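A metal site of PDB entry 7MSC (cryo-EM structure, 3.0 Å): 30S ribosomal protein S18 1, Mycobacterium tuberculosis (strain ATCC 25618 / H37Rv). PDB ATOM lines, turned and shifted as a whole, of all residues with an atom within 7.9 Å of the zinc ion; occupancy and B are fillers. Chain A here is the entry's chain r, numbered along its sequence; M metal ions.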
ATOM      1  N   LYS A  19      20.491 -28.136  -8.601  1.00  0.00           N
ATOM      2  CA  LYS A  19      21.106 -27.884  -7.311  1.00  0.00           C
ATOM      3  C   LYS A  19      20.056 -27.210  -6.428  1.00  0.00           C
ATOM      4  O   LYS A  19      20.118 -27.274  -5.207  1.00  0.00           O
ATOM      5  CB  LYS A  19      22.352 -27.014  -7.467  1.00  0.00           C
ATOM      6  CG  LYS A  19      23.306 -27.064  -6.282  1.00  0.00           C
ATOM      7  CD  LYS A  19      23.113 -25.935  -5.305  1.00  0.00           C
ATOM      8  CE  LYS A  19      24.191 -25.966  -4.236  1.00  0.00           C
ATOM      9  NZ  LYS A  19      24.100 -27.190  -3.413  1.00  0.00           N
ATOM     10  N   CYS A  20      19.099 -26.573  -7.083  1.00  0.00           N
ATOM     11  CA  CYS A  20      17.911 -26.039  -6.423  1.00  0.00           C
ATOM     12  C   CYS A  20      16.823 -27.104  -6.441  1.00  0.00           C
ATOM     13  O   CYS A  20      16.555 -27.699  -7.486  1.00  0.00           O
ATOM     14  CB  CYS A  20      17.425 -24.778  -7.128  1.00  0.00           C
ATOM     15  SG  CYS A  20      15.962 -24.008  -6.427  1.00  0.00           S
ATOM     16  N   VAL A  21      16.206 -27.346  -5.284  1.00  0.00           N
ATOM     17  CA  VAL A  21      15.243 -28.437  -5.186  1.00  0.00           C
ATOM     18  C   VAL A  21      13.932 -28.064  -5.862  1.00  0.00           C
ATOM     19  O   VAL A  21      13.310 -28.878  -6.546  1.00  0.00           O
ATOM     20  CB  VAL A  21      15.033 -28.827  -3.708  1.00  0.00           C
ATOM     21  CG1 VAL A  21      14.030 -29.939  -3.568  1.00  0.00           C
ATOM     22  CG2 VAL A  21      16.353 -29.229  -3.076  1.00  0.00           C
ATOM     23  N   PHE A  22      13.514 -26.803  -5.711  1.00  0.00           N
ATOM     24  CA  PHE A  22      12.229 -26.389  -6.247  1.00  0.00           C
ATOM     25  C   PHE A  22      12.252 -26.243  -7.761  1.00  0.00           C
ATOM     26  O   PHE A  22      11.219 -26.467  -8.419  1.00  0.00           O
ATOM     27  CB  PHE A  22      11.789 -25.080  -5.611  1.00  0.00           C
ATOM     28  CG  PHE A  22      11.509 -25.202  -4.151  1.00  0.00           C
ATOM     29  CD1 PHE A  22      10.316 -25.737  -3.717  1.00  0.00           C
ATOM     30  CD2 PHE A  22      12.424 -24.772  -3.217  1.00  0.00           C
ATOM     31  CE1 PHE A  22      10.053 -25.855  -2.380  1.00  0.00           C
ATOM     32  CE2 PHE A  22      12.162 -24.881  -1.877  1.00  0.00           C
ATOM     33  CZ  PHE A  22      10.969 -25.422  -1.459  1.00  0.00           C
ATOM     34  N   CYS A  23      13.385 -25.851  -8.339  1.00  0.00           N
ATOM     35  CA  CYS A  23      13.456 -25.776  -9.795  1.00  0.00           C
ATOM     36  C   CYS A  23      13.602 -27.140 -10.423  1.00  0.00           C
ATOM     37  O   CYS A  23      13.126 -27.352 -11.548  1.00  0.00           O
ATOM     38  CB  CYS A  23      14.632 -24.891 -10.212  1.00  0.00           C
ATOM     39  SG  CYS A  23      14.456 -23.141  -9.831  1.00  0.00           S
ATOM     40  N   ALA A  24      14.241 -28.088  -9.739  1.00  0.00           N
ATOM     41  CA  ALA A  24      14.441 -29.409 -10.305  1.00  0.00           C
ATOM     42  C   ALA A  24      13.142 -30.196 -10.322  1.00  0.00           C
ATOM     43  O   ALA A  24      12.611 -30.538 -11.387  1.00  0.00           O
ATOM     44  CB  ALA A  24      15.516 -30.161  -9.517  1.00  0.00           C
ATOM     45  N   ILE A  30       4.888 -23.810  -2.835  1.00  0.00           N
ATOM     46  CA  ILE A  30       5.426 -23.306  -1.575  1.00  0.00           C
ATOM     47  C   ILE A  30       4.299 -22.592  -0.858  1.00  0.00           C
ATOM     48  O   ILE A  30       3.824 -21.544  -1.298  1.00  0.00           O
ATOM     49  CB  ILE A  30       6.611 -22.370  -1.807  1.00  0.00           C
ATOM     50  CG1 ILE A  30       7.745 -23.129  -2.477  1.00  0.00           C
ATOM     51  CG2 ILE A  30       7.079 -21.794  -0.504  1.00  0.00           C
ATOM     52  CD1 ILE A  30       8.849 -22.241  -2.967  1.00  0.00           C
ATOM     53  N   GLY A  55      20.913 -23.569  -1.396  1.00  0.00           N
ATOM     54  CA  GLY A  55      21.027 -23.818  -2.816  1.00  0.00           C
ATOM     55  C   GLY A  55      19.885 -23.311  -3.651  1.00  0.00           C
ATOM     56  O   GLY A  55      19.797 -23.664  -4.832  1.00  0.00           O
ATOM     57  N   ASN A  56      18.996 -22.499  -3.083  1.00  0.00           N
ATOM     58  CA  ASN A  56      17.854 -22.008  -3.827  1.00  0.00           C
ATOM     59  C   ASN A  56      18.276 -20.932  -4.823  1.00  0.00           C
ATOM     60  O   ASN A  56      19.367 -20.373  -4.750  1.00  0.00           O
ATOM     61  CB  ASN A  56      16.806 -21.449  -2.873  1.00  0.00           C
ATOM     62  CG  ASN A  56      16.143 -22.517  -2.061  1.00  0.00           C
ATOM     63  OD1 ASN A  56      15.812 -23.581  -2.559  1.00  0.00           O
ATOM     64  ND2 ASN A  56      15.970 -22.239  -0.771  1.00  0.00           N
ATOM     65  N   CYS A  57      17.372 -20.643  -5.757  1.00  0.00           N
ATOM     66  CA  CYS A  57      17.543 -19.545  -6.689  1.00  0.00           C
ATOM     67  C   CYS A  57      16.966 -18.279  -6.072  1.00  0.00           C
ATOM     68  O   CYS A  57      16.548 -18.258  -4.909  1.00  0.00           O
ATOM     69  CB  CYS A  57      16.891 -19.900  -8.020  1.00  0.00           C
ATOM     70  SG  CYS A  57      15.109 -20.129  -7.931  1.00  0.00           S
ATOM     71  N   VAL A  58      16.931 -17.190  -6.842  1.00  0.00           N
ATOM     72  CA  VAL A  58      16.437 -15.930  -6.284  1.00  0.00           C
ATOM     73  C   VAL A  58      14.924 -15.944  -6.212  1.00  0.00           C
ATOM     74  O   VAL A  58      14.325 -15.406  -5.273  1.00  0.00           O
ATOM     75  CB  VAL A  58      16.952 -14.755  -7.125  1.00  0.00           C
ATOM     76  CG1 VAL A  58      16.551 -13.419  -6.515  1.00  0.00           C
ATOM     77  CG2 VAL A  58      18.432 -14.827  -7.292  1.00  0.00           C
ATOM     78  N   GLN A  59      14.264 -16.578  -7.187  1.00  0.00           N
ATOM     79  CA  GLN A  59      12.817 -16.503  -7.253  1.00  0.00           C
ATOM     80  C   GLN A  59      12.152 -17.355  -6.179  1.00  0.00           C
ATOM     81  O   GLN A  59      11.068 -17.018  -5.713  1.00  0.00           O
ATOM     82  CB  GLN A  59      12.328 -16.924  -8.624  1.00  0.00           C
ATOM     83  CG  GLN A  59      12.779 -16.006  -9.721  1.00  0.00           C
ATOM     84  CD  GLN A  59      12.265 -16.445 -11.063  1.00  0.00           C
ATOM     85  OE1 GLN A  59      11.580 -17.452 -11.181  1.00  0.00           O
ATOM     86  NE2 GLN A  59      12.595 -15.680 -12.090  1.00  0.00           N
ATOM     87  N   HIS A  60      12.785 -18.448  -5.781  1.00  0.00           N
ATOM     88  CA  HIS A  60      12.195 -19.298  -4.759  1.00  0.00           C
ATOM     89  C   HIS A  60      12.621 -18.919  -3.347  1.00  0.00           C
ATOM     90  O   HIS A  60      11.876 -19.218  -2.410  1.00  0.00           O
ATOM     91  CB  HIS A  60      12.546 -20.767  -5.013  1.00  0.00           C
ATOM     92  CG  HIS A  60      11.857 -21.348  -6.205  1.00  0.00           C
ATOM     93  ND1 HIS A  60      12.448 -21.426  -7.442  1.00  0.00           N
ATOM     94  CD2 HIS A  60      10.605 -21.840  -6.348  1.00  0.00           C
ATOM     95  CE1 HIS A  60      11.598 -21.975  -8.293  1.00  0.00           C
ATOM     96  NE2 HIS A  60      10.475 -22.228  -7.653  1.00  0.00           N
ATOM     97  N   GLN A  61      13.772 -18.285  -3.181  1.00  0.00           N
ATOM     98  CA  GLN A  61      14.177 -17.793  -1.864  1.00  0.00           C
ATOM     99  C   GLN A  61      13.247 -16.694  -1.387  1.00  0.00           C
ATOM    100  O   GLN A  61      12.987 -16.586  -0.184  1.00  0.00           O
ATOM    101  CB  GLN A  61      15.614 -17.305  -1.911  1.00  0.00           C
ATOM    102  CG  GLN A  61      16.171 -16.874  -0.582  1.00  0.00           C
ATOM    103  CD  GLN A  61      16.317 -18.025   0.358  1.00  0.00           C
ATOM    104  OE1 GLN A  61      16.686 -19.129  -0.042  1.00  0.00           O
ATOM    105  NE2 GLN A  61      16.030 -17.798   1.621  1.00  0.00           N
HETATM  106 ZN    ZN M   1      14.371 -22.417  -7.468  1.00  0.00          ZN
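SG of Cys 57 sits close to N of Gln 59 (3.7 Å).
The side-chain sulfur (SG) of Cys 20 sits close to the backbone NH (N) of Phe 22 (3.8 Å).
The nearest printed residue that does not touch the zinc ion is Phe 22 (4.1 Å).
The zinc ion is bound by ND1 of His 60 (2.2 Å), SG of Cys 57 (2.4 Å), SG of Cys 23 (2.5 Å) and SG of Cys 20 (2.5 Å).
The zinc ion has four donor atoms within binding distance.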
